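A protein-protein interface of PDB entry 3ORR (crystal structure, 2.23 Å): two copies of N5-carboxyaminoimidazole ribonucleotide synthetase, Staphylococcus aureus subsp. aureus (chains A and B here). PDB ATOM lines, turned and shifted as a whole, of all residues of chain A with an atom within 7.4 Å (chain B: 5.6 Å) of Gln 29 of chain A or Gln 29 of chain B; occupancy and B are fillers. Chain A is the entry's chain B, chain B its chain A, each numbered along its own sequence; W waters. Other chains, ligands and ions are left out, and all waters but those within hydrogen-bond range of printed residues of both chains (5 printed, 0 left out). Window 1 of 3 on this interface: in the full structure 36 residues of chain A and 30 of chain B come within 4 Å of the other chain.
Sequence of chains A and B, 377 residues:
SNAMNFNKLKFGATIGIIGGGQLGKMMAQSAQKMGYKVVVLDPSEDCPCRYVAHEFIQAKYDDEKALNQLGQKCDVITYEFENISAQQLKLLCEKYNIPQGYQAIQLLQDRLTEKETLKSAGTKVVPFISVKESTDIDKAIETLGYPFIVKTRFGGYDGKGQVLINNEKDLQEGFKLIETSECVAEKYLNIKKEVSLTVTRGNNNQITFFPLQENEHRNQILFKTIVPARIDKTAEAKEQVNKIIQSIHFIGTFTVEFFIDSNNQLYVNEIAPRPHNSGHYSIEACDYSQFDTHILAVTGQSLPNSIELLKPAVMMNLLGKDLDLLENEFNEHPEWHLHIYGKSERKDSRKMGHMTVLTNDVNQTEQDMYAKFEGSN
The side-chain amino group (NZ) of Lys 25 of chain B lies within hydrogen-bond range of the backbone carbonyl oxygen (O) of Gln 32 of chain A (2.6 Å).
The side-chain amide nitrogen (NE2) of Gln 29 of chain A lies close to the side-chain amide nitrogen (NE2) of Gln 29 of chain B (2.6 Å).
O of Gln 32 of chain B sits at hydrogen-bond distance from NZ of Lys 25 of chain A.
O of Tyr 51 of chain A sits at hydrogen-bond distance from NE2 of Gln 32 of chain B (3.0 Å).
NE2 of Gln 32 of chain B is in hydrogen-bond range of O of Val 52 of chain B (2.8 Å).
The side-chain sulfur of Cys 49 of chain A lies close to the backbone NH of Lys 25 of chain A (3.6 Å).
The side-chain amide oxygen (OE1) of Gln 32 of chain A lies close to the backbone carbonyl oxygen (O) of Val 52 of chain A (3.0 Å).
Among the printed residues, merely in contact across the chains: Gln 29 of chain A with Lys 33 of chain B (3.7 Å), Gln 32 of chain A with Val 52 of chain B (3.6 Å), Tyr 51 of chain A with Val 52 of chain B (3.4 Å) and Val 52 of chain A with Gln 32 of chain B (3.4 Å).
Gln 29 of chain A touches just these residues of chain B: Gln 29 (2.6 Å) and Lys 33 (3.7 Å).
Gln 29 of chain B touches just one residue of chain A: Gln 29 (2.6 Å).
Of the printed residues of chain A, Val 52 of chain B touches Gln 32 (3.6 Å) and Tyr 51 (3.4 Å).
Of the printed residues of chain A, Lys 33 of chain B touches Gln 29 (3.7 Å).
Of the printed residues of chain B, Tyr 51 of chain A touches Gln 32 and Val 52.
Of the printed residues of chain B, Gln 32 of chain A touches Lys 25 and Val 52.
Printed residues of chain A within 4 Å of Gln 32 of chain B: Lys 25 (2.6 Å), Tyr 51 (3.0 Å) and Val 52 (3.4 Å).
Cys 49 of chain A touches none of the printed residues of chain B.
Ala 31 of chain B touches none of the printed residues of chain A.
The nearest residue of chain A that does not touch Gln 29 of chain B is Lys 33 of chain A (4.2 Å).
Hydrophobic or aromatic side chains of chain B that line the printed part of chain A: Val 52.
Lys 25 of chain A touches Gln 32 of chain B, and with the chains exchanged Gln 32 of chain A touches Lys 25 of chain B.
Gln 29 of chain A touches its own counterpart, Gln 29 of chain B.
Gln 29 of chain A touches Lys 33 of chain B, but with the chains exchanged Lys 33 of chain A does not touch Gln 29 of chain B (4.2 Å).
Gln 32 of chain A touches Val 52 of chain B, and with the chains exchanged Val 52 of chain A touches Gln 32 of chain B.
Positions printed for both chains: 24, 25, 26, 27, 28, 29, 30, 31, 32, 33, 34 and 52.
Of the 8 pairs that touch across the chains among the printed residues, 5 have their exchanged pair printed and touching as well.
Water W2 lies within hydrogen-bond range of the side-chain amide nitrogen (NE2) of Gln 32 of chain A (2.6 Å) and the side-chain amino group (NZ) of Lys 25 of chain B (3.2 Å).
Water W3 lies within hydrogen-bond range of the side-chain amino group (NZ) of Lys 25 of chain B (2.7 Å) and the backbone carbonyl oxygen (O) of Lys 33 of chain A (2.7 Å).
Water W5 lies within hydrogen-bond range of the side-chain amino group (NZ) of Lys 25 of chain A (2.7 Å) and the backbone carbonyl oxygen (O) of Lys 33 of chain B (2.9 Å).
Water W4 bridges the side-chain amide oxygen (OE1) of Gln 32 of chain B (2.7 Å) and the side-chain amino group (NZ) of Lys 25 of chain A (3.2 Å).
Water W1 lies within hydrogen-bond range of the backbone NH of Tyr 51 of chain A (2.8 Å) and the side-chain amide oxygen of Gln 32 of chain B (2.9 Å).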
ATOM      1  N   ILE A  17      28.841 -11.540 -20.909  1.00  0.00           N
ATOM      2  CA  ILE A  17      29.982 -12.357 -20.482  1.00  0.00           C
ATOM      3  C   ILE A  17      30.933 -12.510 -21.645  1.00  0.00           C
ATOM      4  O   ILE A  17      30.539 -12.991 -22.709  1.00  0.00           O
ATOM      5  CB  ILE A  17      29.557 -13.720 -19.986  1.00  0.00           C
ATOM      6  CG1 ILE A  17      28.690 -13.603 -18.737  1.00  0.00           C
ATOM      7  CG2 ILE A  17      30.778 -14.590 -19.678  1.00  0.00           C
ATOM      8  CD1 ILE A  17      27.793 -14.919 -18.499  1.00  0.00           C
ATOM      9  N   LEU A  23      33.192 -21.638 -16.982  1.00  0.00           N
ATOM     10  CA  LEU A  23      33.119 -20.569 -16.014  1.00  0.00           C
ATOM     11  C   LEU A  23      32.048 -19.576 -16.448  1.00  0.00           C
ATOM     12  O   LEU A  23      31.173 -19.213 -15.643  1.00  0.00           O
ATOM     13  CB  LEU A  23      34.479 -19.882 -15.851  1.00  0.00           C
ATOM     14  CG  LEU A  23      35.633 -20.827 -15.457  1.00  0.00           C
ATOM     15  CD1 LEU A  23      36.951 -20.010 -15.340  1.00  0.00           C
ATOM     16  CD2 LEU A  23      35.353 -21.571 -14.150  1.00  0.00           C
ATOM     17  N   GLY A  24      32.074 -19.179 -17.724  1.00  0.00           N
ATOM     18  CA  GLY A  24      30.955 -18.398 -18.249  1.00  0.00           C
ATOM     19  C   GLY A  24      29.619 -19.099 -18.011  1.00  0.00           C
ATOM     20  O   GLY A  24      28.646 -18.470 -17.586  1.00  0.00           O
ATOM     21  N   LYS A  25      29.557 -20.402 -18.272  1.00  0.00           N
ATOM     22  CA  LYS A  25      28.282 -21.131 -18.134  1.00  0.00           C
ATOM     23  C   LYS A  25      27.738 -21.023 -16.710  1.00  0.00           C
ATOM     24  O   LYS A  25      26.568 -20.713 -16.508  1.00  0.00           O
ATOM     25  CB  LYS A  25      28.439 -22.604 -18.487  1.00  0.00           C
ATOM     26  CG  LYS A  25      27.172 -23.474 -18.283  1.00  0.00           C
ATOM     27  CD  LYS A  25      27.504 -24.944 -18.391  1.00  0.00           C
ATOM     28  CE  LYS A  25      26.250 -25.819 -18.543  1.00  0.00           C
ATOM     29  NZ  LYS A  25      26.606 -27.275 -18.402  1.00  0.00           N
ATOM     30  N   MET A  26      28.596 -21.261 -15.727  1.00  0.00           N
ATOM     31  CA  MET A  26      28.141 -21.252 -14.349  1.00  0.00           C
ATOM     32  C   MET A  26      27.751 -19.842 -13.847  1.00  0.00           C
ATOM     33  O   MET A  26      26.864 -19.715 -12.978  1.00  0.00           O
ATOM     34  CB  MET A  26      29.150 -21.972 -13.451  1.00  0.00           C
ATOM     35  CG  MET A  26      29.331 -23.487 -13.824  1.00  0.00           C
ATOM     36  SD  MET A  26      30.542 -24.447 -12.651  1.00  0.00           S
ATOM     37  CE  MET A  26      32.007 -24.284 -13.855  1.00  0.00           C
ATOM     38  N   MET A  27      28.378 -18.808 -14.413  1.00  0.00           N
ATOM     39  CA  MET A  27      27.994 -17.436 -14.120  1.00  0.00           C
ATOM     40  C   MET A  27      26.610 -17.179 -14.692  1.00  0.00           C
ATOM     41  O   MET A  27      25.749 -16.546 -14.034  1.00  0.00           O
ATOM     42  CB  MET A  27      28.913 -16.402 -14.798  1.00  0.00           C
ATOM     43  CG  MET A  27      30.316 -16.254 -14.321  1.00  0.00           C
ATOM     44  SD  MET A  27      31.198 -14.821 -15.379  1.00  0.00           S
ATOM     45  CE  MET A  27      32.899 -14.857 -14.434  1.00  0.00           C
ATOM     46  N   ALA A  28      26.417 -17.622 -15.932  1.00  0.00           N
ATOM     47  CA  ALA A  28      25.169 -17.422 -16.636  1.00  0.00           C
ATOM     48  C   ALA A  28      24.043 -18.130 -15.834  1.00  0.00           C
ATOM     49  O   ALA A  28      22.948 -17.578 -15.756  1.00  0.00           O
ATOM     50  CB  ALA A  28      25.237 -17.948 -18.020  1.00  0.00           C
ATOM     51  N   GLN A  29      24.326 -19.294 -15.227  1.00  0.00           N
ATOM     52  CA  GLN A  29      23.275 -20.049 -14.543  1.00  0.00           C
ATOM     53  C   GLN A  29      22.814 -19.336 -13.259  1.00  0.00           C
ATOM     54  O   GLN A  29      21.604 -19.253 -12.972  1.00  0.00           O
ATOM     55  CB  GLN A  29      23.715 -21.474 -14.208  1.00  0.00           C
ATOM     56  CG  GLN A  29      23.833 -22.382 -15.427  1.00  0.00           C
ATOM     57  CD  GLN A  29      22.750 -23.440 -15.419  1.00  0.00           C
ATOM     58  OE1 GLN A  29      23.036 -24.630 -15.324  1.00  0.00           O
ATOM     59  NE2 GLN A  29      21.469 -22.994 -15.473  1.00  0.00           N
ATOM     60  N   SER A  30      23.774 -18.817 -12.500  1.00  0.00           N
ATOM     61  CA  SER A  30      23.440 -17.962 -11.365  1.00  0.00           C
ATOM     62  C   SER A  30      22.665 -16.744 -11.829  1.00  0.00           C
ATOM     63  O   SER A  30      21.622 -16.394 -11.237  1.00  0.00           O
ATOM     64  CB  SER A  30      24.709 -17.497 -10.673  1.00  0.00           C
ATOM     65  OG  SER A  30      25.229 -18.532  -9.874  1.00  0.00           O
ATOM     66  N   ALA A  31      23.161 -16.088 -12.879  1.00  0.00           N
ATOM     67  CA  ALA A  31      22.566 -14.850 -13.350  1.00  0.00           C
ATOM     68  C   ALA A  31      21.069 -15.052 -13.665  1.00  0.00           C
ATOM     69  O   ALA A  31      20.220 -14.228 -13.257  1.00  0.00           O
ATOM     70  CB  ALA A  31      23.314 -14.321 -14.569  1.00  0.00           C
ATOM     71  N   GLN A  32      20.747 -16.141 -14.371  1.00  0.00           N
ATOM     72  CA  GLN A  32      19.349 -16.387 -14.769  1.00  0.00           C
ATOM     73  C   GLN A  32      18.524 -16.785 -13.586  1.00  0.00           C
ATOM     74  O   GLN A  32      17.327 -16.465 -13.524  1.00  0.00           O
ATOM     75  CB  GLN A  32      19.215 -17.468 -15.846  1.00  0.00           C
ATOM     76  CG  GLN A  32      19.788 -17.081 -17.174  1.00  0.00           C
ATOM     77  CD  GLN A  32      18.951 -17.616 -18.326  1.00  0.00           C
ATOM     78  OE1 GLN A  32      19.495 -17.947 -19.369  1.00  0.00           O
ATOM     79  NE2 GLN A  32      17.627 -17.653 -18.161  1.00  0.00           N
ATOM     80  N   LYS A  33      19.153 -17.484 -12.646  1.00  0.00           N
ATOM     81  CA  LYS A  33      18.457 -17.867 -11.449  1.00  0.00           C
ATOM     82  C   LYS A  33      17.940 -16.591 -10.755  1.00  0.00           C
ATOM     83  O   LYS A  33      16.793 -16.555 -10.276  1.00  0.00           O
ATOM     84  CB  LYS A  33      19.375 -18.652 -10.517  1.00  0.00           C
ATOM     85  CG  LYS A  33      18.795 -18.835  -9.137  1.00  0.00           C
ATOM     86  CD  LYS A  33      19.747 -19.618  -8.209  1.00  0.00           C
ATOM     87  CE  LYS A  33      21.110 -18.903  -8.085  1.00  0.00           C
ATOM     88  NZ  LYS A  33      22.087 -19.674  -7.185  1.00  0.00           N
ATOM     89  N   MET A  34      18.803 -15.560 -10.753  1.00  0.00           N
ATOM     90  CA  MET A  34      18.577 -14.337 -10.045  1.00  0.00           C
ATOM     91  C   MET A  34      17.811 -13.326 -10.893  1.00  0.00           C
ATOM     92  O   MET A  34      17.590 -12.208 -10.473  1.00  0.00           O
ATOM     93  CB  MET A  34      19.914 -13.762  -9.594  1.00  0.00           C
ATOM     94  CG  MET A  34      20.720 -14.738  -8.781  1.00  0.00           C
ATOM     95  SD  MET A  34      22.637 -14.270  -8.699  1.00  0.00           S
ATOM     96  CE  MET A  34      22.354 -12.883  -7.441  1.00  0.00           C
ATOM     97  N   GLY A  35      17.457 -13.712 -12.109  1.00  0.00           N
ATOM     98  CA  GLY A  35      16.553 -12.942 -12.925  1.00  0.00           C
ATOM     99  C   GLY A  35      17.253 -11.908 -13.752  1.00  0.00           C
ATOM    100  O   GLY A  35      16.638 -10.924 -14.162  1.00  0.00           O
ATOM    101  N   TYR A  36      18.524 -12.119 -14.045  1.00  0.00           N
ATOM    102  CA  TYR A  36      19.240 -11.264 -14.986  1.00  0.00           C
ATOM    103  C   TYR A  36      19.257 -11.912 -16.340  1.00  0.00           C
ATOM    104  O   TYR A  36      19.344 -13.149 -16.443  1.00  0.00           O
ATOM    105  CB  TYR A  36      20.691 -11.031 -14.498  1.00  0.00           C
ATOM    106  CG  TYR A  36      20.741 -10.206 -13.241  1.00  0.00           C
ATOM    107  CD1 TYR A  36      20.637  -8.802 -13.314  1.00  0.00           C
ATOM    108  CD2 TYR A  36      20.807 -10.809 -11.970  1.00  0.00           C
ATOM    109  CE1 TYR A  36      20.630  -8.015 -12.157  1.00  0.00           C
ATOM    110  CE2 TYR A  36      20.788 -10.018 -10.805  1.00  0.00           C
ATOM    111  CZ  TYR A  36      20.728  -8.639 -10.914  1.00  0.00           C
ATOM    112  OH  TYR A  36      20.717  -7.861  -9.805  1.00  0.00           O
ATOM    113  N   VAL A  38      21.183 -12.670 -19.928  1.00  0.00           N
ATOM    114  CA  VAL A  38      22.581 -12.986 -20.229  1.00  0.00           C
ATOM    115  C   VAL A  38      22.915 -12.929 -21.710  1.00  0.00           C
ATOM    116  O   VAL A  38      22.289 -13.605 -22.507  1.00  0.00           O
ATOM    117  CB  VAL A  38      22.928 -14.426 -19.718  1.00  0.00           C
ATOM    118  CG1 VAL A  38      24.273 -14.850 -20.211  1.00  0.00           C
ATOM    119  CG2 VAL A  38      22.860 -14.479 -18.188  1.00  0.00           C
ATOM    120  N   CYS A  49      28.490 -22.293 -22.668  1.00  0.00           N
ATOM    121  CA  CYS A  49      27.601 -21.278 -22.099  1.00  0.00           C
ATOM    122  C   CYS A  49      26.466 -20.864 -23.075  1.00  0.00           C
ATOM    123  O   CYS A  49      25.487 -20.199 -22.684  1.00  0.00           O
ATOM    124  CB  CYS A  49      28.425 -20.045 -21.676  1.00  0.00           C
ATOM    125  SG  CYS A  49      27.479 -18.787 -20.781  1.00  0.00           S
ATOM    126  N   TYR A  51      23.673 -22.072 -24.420  1.00  0.00           N
ATOM    127  CA  TYR A  51      22.227 -22.261 -24.300  1.00  0.00           C
ATOM    128  C   TYR A  51      21.711 -21.965 -22.913  1.00  0.00           C
ATOM    129  O   TYR A  51      20.639 -22.414 -22.542  1.00  0.00           O
ATOM    130  CB  TYR A  51      21.785 -23.636 -24.805  1.00  0.00           C
ATOM    131  CG  TYR A  51      22.121 -23.807 -26.278  1.00  0.00           C
ATOM    132  CD1 TYR A  51      21.321 -23.182 -27.265  1.00  0.00           C
ATOM    133  CD2 TYR A  51      23.221 -24.562 -26.681  1.00  0.00           C
ATOM    134  CE1 TYR A  51      21.637 -23.291 -28.648  1.00  0.00           C
ATOM    135  CE2 TYR A  51      23.543 -24.712 -28.066  1.00  0.00           C
ATOM    136  CZ  TYR A  51      22.754 -24.049 -29.034  1.00  0.00           C
ATOM    137  OH  TYR A  51      23.067 -24.153 -30.363  1.00  0.00           O
ATOM    138  N   VAL A  52      22.497 -21.222 -22.143  1.00  0.00           N
ATOM    139  CA  VAL A  52      22.004 -20.589 -20.941  1.00  0.00           C
ATOM    140  C   VAL A  52      22.197 -19.069 -21.079  1.00  0.00           C
ATOM    141  O   VAL A  52      22.386 -18.339 -20.094  1.00  0.00           O
ATOM    142  CB  VAL A  52      22.727 -21.173 -19.684  1.00  0.00           C
ATOM    143  CG1 VAL A  52      22.231 -22.623 -19.388  1.00  0.00           C
ATOM    144  CG2 VAL A  52      24.235 -21.156 -19.865  1.00  0.00           C
ATOM    145  N   PHE A 291      30.059 -18.233  -7.779  1.00  0.00           N
ATOM    146  CA  PHE A 291      29.314 -17.666  -8.909  1.00  0.00           C
ATOM    147  C   PHE A 291      28.170 -16.794  -8.447  1.00  0.00           C
ATOM    148  O   PHE A 291      27.951 -15.711  -9.026  1.00  0.00           O
ATOM    149  CB  PHE A 291      28.835 -18.782  -9.842  1.00  0.00           C
ATOM    150  CG  PHE A 291      29.981 -19.572 -10.429  1.00  0.00           C
ATOM    151  CD1 PHE A 291      30.733 -19.031 -11.475  1.00  0.00           C
ATOM    152  CD2 PHE A 291      30.336 -20.828  -9.893  1.00  0.00           C
ATOM    153  CE1 PHE A 291      31.785 -19.742 -11.992  1.00  0.00           C
ATOM    154  CE2 PHE A 291      31.362 -21.558 -10.423  1.00  0.00           C
ATOM    155  CZ  PHE A 291      32.103 -21.014 -11.457  1.00  0.00           C
ATOM    156  N   ASP A 292      27.464 -17.241  -7.393  1.00  0.00           N
ATOM    157  CA  ASP A 292      26.407 -16.418  -6.823  1.00  0.00           C
ATOM    158  C   ASP A 292      26.973 -15.057  -6.392  1.00  0.00           C
ATOM    159  O   ASP A 292      26.442 -14.027  -6.754  1.00  0.00           O
ATOM    160  CB  ASP A 292      25.703 -17.064  -5.642  1.00  0.00           C
ATOM    161  CG  ASP A 292      25.039 -18.395  -5.992  1.00  0.00           C
ATOM    162  OD1 ASP A 292      24.474 -18.537  -7.130  1.00  0.00           O
ATOM    163  OD2 ASP A 292      25.073 -19.269  -5.088  1.00  0.00           O
ATOM    164  N   ILE A 295      28.013 -12.491  -9.146  1.00  0.00           N
ATOM    165  CA  ILE A 295      26.921 -11.791  -9.830  1.00  0.00           C
ATOM    166  C   ILE A 295      26.405 -10.667  -8.911  1.00  0.00           C
ATOM    167  O   ILE A 295      26.103  -9.573  -9.391  1.00  0.00           O
ATOM    168  CB  ILE A 295      25.715 -12.717 -10.133  1.00  0.00           C
ATOM    169  CG1 ILE A 295      26.084 -13.841 -11.116  1.00  0.00           C
ATOM    170  CG2 ILE A 295      24.509 -11.882 -10.588  1.00  0.00           C
ATOM    171  CD1 ILE A 295      26.562 -13.320 -12.523  1.00  0.00           C
ATOM    172  N   GLY B  24       9.781 -25.767 -15.030  1.00  0.00           N
ATOM    173  CA  GLY B  24      10.582 -26.345 -16.090  1.00  0.00           C
ATOM    174  C   GLY B  24      11.924 -25.656 -16.176  1.00  0.00           C
ATOM    175  O   GLY B  24      12.949 -26.298 -16.518  1.00  0.00           O
ATOM    176  N   LYS B  25      11.929 -24.354 -15.872  1.00  0.00           N
ATOM    177  CA  LYS B  25      13.176 -23.567 -15.868  1.00  0.00           C
ATOM    178  C   LYS B  25      14.178 -24.226 -14.948  1.00  0.00           C
ATOM    179  O   LYS B  25      15.275 -24.536 -15.334  1.00  0.00           O
ATOM    180  CB  LYS B  25      12.949 -22.099 -15.407  1.00  0.00           C
ATOM    181  CG  LYS B  25      14.247 -21.322 -15.161  1.00  0.00           C
ATOM    182  CD  LYS B  25      13.989 -19.924 -14.567  1.00  0.00           C
ATOM    183  CE  LYS B  25      15.171 -18.989 -14.792  1.00  0.00           C
ATOM    184  NZ  LYS B  25      15.076 -17.763 -14.026  1.00  0.00           N
ATOM    185  N   MET B  26      13.765 -24.438 -13.720  1.00  0.00           N
ATOM    186  CA  MET B  26      14.637 -24.988 -12.742  1.00  0.00           C
ATOM    187  C   MET B  26      15.039 -26.437 -13.067  1.00  0.00           C
ATOM    188  O   MET B  26      16.159 -26.847 -12.735  1.00  0.00           O
ATOM    189  CB  MET B  26      14.004 -24.866 -11.349  1.00  0.00           C
ATOM    190  CG  MET B  26      13.988 -23.418 -10.832  1.00  0.00           C
ATOM    191  SD  MET B  26      13.102 -23.140  -9.077  1.00  0.00           S
ATOM    192  CE  MET B  26      11.251 -23.165  -9.711  1.00  0.00           C
ATOM    193  N   MET B  27      14.149 -27.201 -13.693  1.00  0.00           N
ATOM    194  CA  MET B  27      14.478 -28.555 -14.165  1.00  0.00           C
ATOM    195  C   MET B  27      15.607 -28.462 -15.152  1.00  0.00           C
ATOM    196  O   MET B  27      16.572 -29.202 -15.062  1.00  0.00           O
ATOM    197  CB  MET B  27      13.281 -29.213 -14.888  1.00  0.00           C
ATOM    198  CG  MET B  27      12.142 -29.721 -14.011  1.00  0.00           C
ATOM    199  SD  MET B  27      10.778 -30.570 -15.144  1.00  0.00           S
ATOM    200  CE  MET B  27       9.542 -31.158 -13.733  1.00  0.00           C
ATOM    201  N   ALA B  28      15.454 -27.549 -16.113  1.00  0.00           N
ATOM    202  CA  ALA B  28      16.373 -27.411 -17.211  1.00  0.00           C
ATOM    203  C   ALA B  28      17.749 -26.973 -16.751  1.00  0.00           C
ATOM    204  O   ALA B  28      18.775 -27.408 -17.311  1.00  0.00           O
ATOM    205  CB  ALA B  28      15.803 -26.419 -18.280  1.00  0.00           C
ATOM    206  N   GLN B  29      17.787 -26.101 -15.747  1.00  0.00           N
ATOM    207  CA  GLN B  29      19.110 -25.685 -15.205  1.00  0.00           C
ATOM    208  C   GLN B  29      19.806 -26.869 -14.508  1.00  0.00           C
ATOM    209  O   GLN B  29      21.009 -27.078 -14.690  1.00  0.00           O
ATOM    210  CB  GLN B  29      18.994 -24.489 -14.269  1.00  0.00           C
ATOM    211  CG  GLN B  29      18.443 -23.266 -14.982  1.00  0.00           C
ATOM    212  CD  GLN B  29      18.624 -21.969 -14.218  1.00  0.00           C
ATOM    213  OE1 GLN B  29      17.676 -21.420 -13.630  1.00  0.00           O
ATOM    214  NE2 GLN B  29      19.815 -21.481 -14.204  1.00  0.00           N
ATOM    215  N   SER B  30      19.039 -27.686 -13.766  1.00  0.00           N
ATOM    216  CA  SER B  30      19.649 -28.903 -13.207  1.00  0.00           C
ATOM    217  C   SER B  30      20.174 -29.764 -14.358  1.00  0.00           C
ATOM    218  O   SER B  30      21.315 -30.211 -14.339  1.00  0.00           O
ATOM    219  CB  SER B  30      18.645 -29.711 -12.377  1.00  0.00           C
ATOM    220  OG  SER B  30      18.724 -29.327 -11.019  1.00  0.00           O
ATOM    221  N   ALA B  31      19.314 -30.004 -15.335  1.00  0.00           N
ATOM    222  CA  ALA B  31      19.691 -30.788 -16.497  1.00  0.00           C
ATOM    223  C   ALA B  31      20.986 -30.277 -17.165  1.00  0.00           C
ATOM    224  O   ALA B  31      21.852 -31.069 -17.485  1.00  0.00           O
ATOM    225  CB  ALA B  31      18.530 -30.852 -17.518  1.00  0.00           C
ATOM    226  N   GLN B  32      21.096 -28.971 -17.453  1.00  0.00           N
ATOM    227  CA  GLN B  32      22.299 -28.497 -18.222  1.00  0.00           C
ATOM    228  C   GLN B  32      23.534 -28.564 -17.343  1.00  0.00           C
ATOM    229  O   GLN B  32      24.604 -28.893 -17.808  1.00  0.00           O
ATOM    230  CB  GLN B  32      22.124 -27.085 -18.784  1.00  0.00           C
ATOM    231  CG  GLN B  32      21.130 -27.012 -19.961  1.00  0.00           C
ATOM    232  CD  GLN B  32      21.392 -25.830 -20.852  1.00  0.00           C
ATOM    233  OE1 GLN B  32      22.537 -25.531 -21.191  1.00  0.00           O
ATOM    234  NE2 GLN B  32      20.328 -25.128 -21.228  1.00  0.00           N
ATOM    235  N   LYS B  33      23.387 -28.260 -16.058  1.00  0.00           N
ATOM    236  CA  LYS B  33      24.454 -28.527 -15.092  1.00  0.00           C
ATOM    237  C   LYS B  33      25.011 -29.968 -15.223  1.00  0.00           C
ATOM    238  O   LYS B  33      26.206 -30.179 -15.158  1.00  0.00           O
ATOM    239  CB  LYS B  33      23.975 -28.287 -13.656  1.00  0.00           C
ATOM    240  CG  LYS B  33      25.022 -28.675 -12.604  1.00  0.00           C
ATOM    241  CD  LYS B  33      24.479 -28.392 -11.220  1.00  0.00           C
ATOM    242  CE  LYS B  33      23.314 -29.368 -10.848  1.00  0.00           C
ATOM    243  NZ  LYS B  33      22.815 -29.205  -9.404  1.00  0.00           N
ATOM    244  N   MET B  34      24.126 -30.921 -15.431  1.00  0.00           N
ATOM    245  CA  MET B  34      24.465 -32.357 -15.468  1.00  0.00           C
ATOM    246  C   MET B  34      24.874 -32.833 -16.856  1.00  0.00           C
ATOM    247  O   MET B  34      25.050 -34.020 -17.092  1.00  0.00           O
ATOM    248  CB  MET B  34      23.232 -33.167 -14.959  1.00  0.00           C
ATOM    249  CG  MET B  34      22.954 -32.790 -13.458  1.00  0.00           C
ATOM    250  SD  MET B  34      21.171 -33.320 -12.823  1.00  0.00           S
ATOM    251  CE  MET B  34      21.770 -35.098 -12.646  1.00  0.00           C
ATOM    252  N   VAL B  52      17.053 -21.228 -21.073  1.00  0.00           N
ATOM    253  CA  VAL B  52      17.872 -22.318 -20.521  1.00  0.00           C
ATOM    254  C   VAL B  52      17.568 -23.638 -21.218  1.00  0.00           C
ATOM    255  O   VAL B  52      17.641 -24.700 -20.615  1.00  0.00           O
ATOM    256  CB  VAL B  52      17.658 -22.431 -19.026  1.00  0.00           C
ATOM    257  CG1 VAL B  52      18.326 -21.237 -18.329  1.00  0.00           C
ATOM    258  CG2 VAL B  52      16.204 -22.519 -18.707  1.00  0.00           C
HETATM  259  O   HOH W   1      24.599 -24.096 -22.676  1.00  0.00           O
HETATM  260  O   HOH W   2      15.976 -16.277 -16.724  1.00  0.00           O
HETATM  261  O   HOH W   3      14.878 -18.050 -11.399  1.00  0.00           O
HETATM  262  O   HOH W   4      24.562 -27.352 -20.922  1.00  0.00           O
HETATM  263  O   HOH W   5      27.944 -28.134 -16.241  1.00  0.00           O
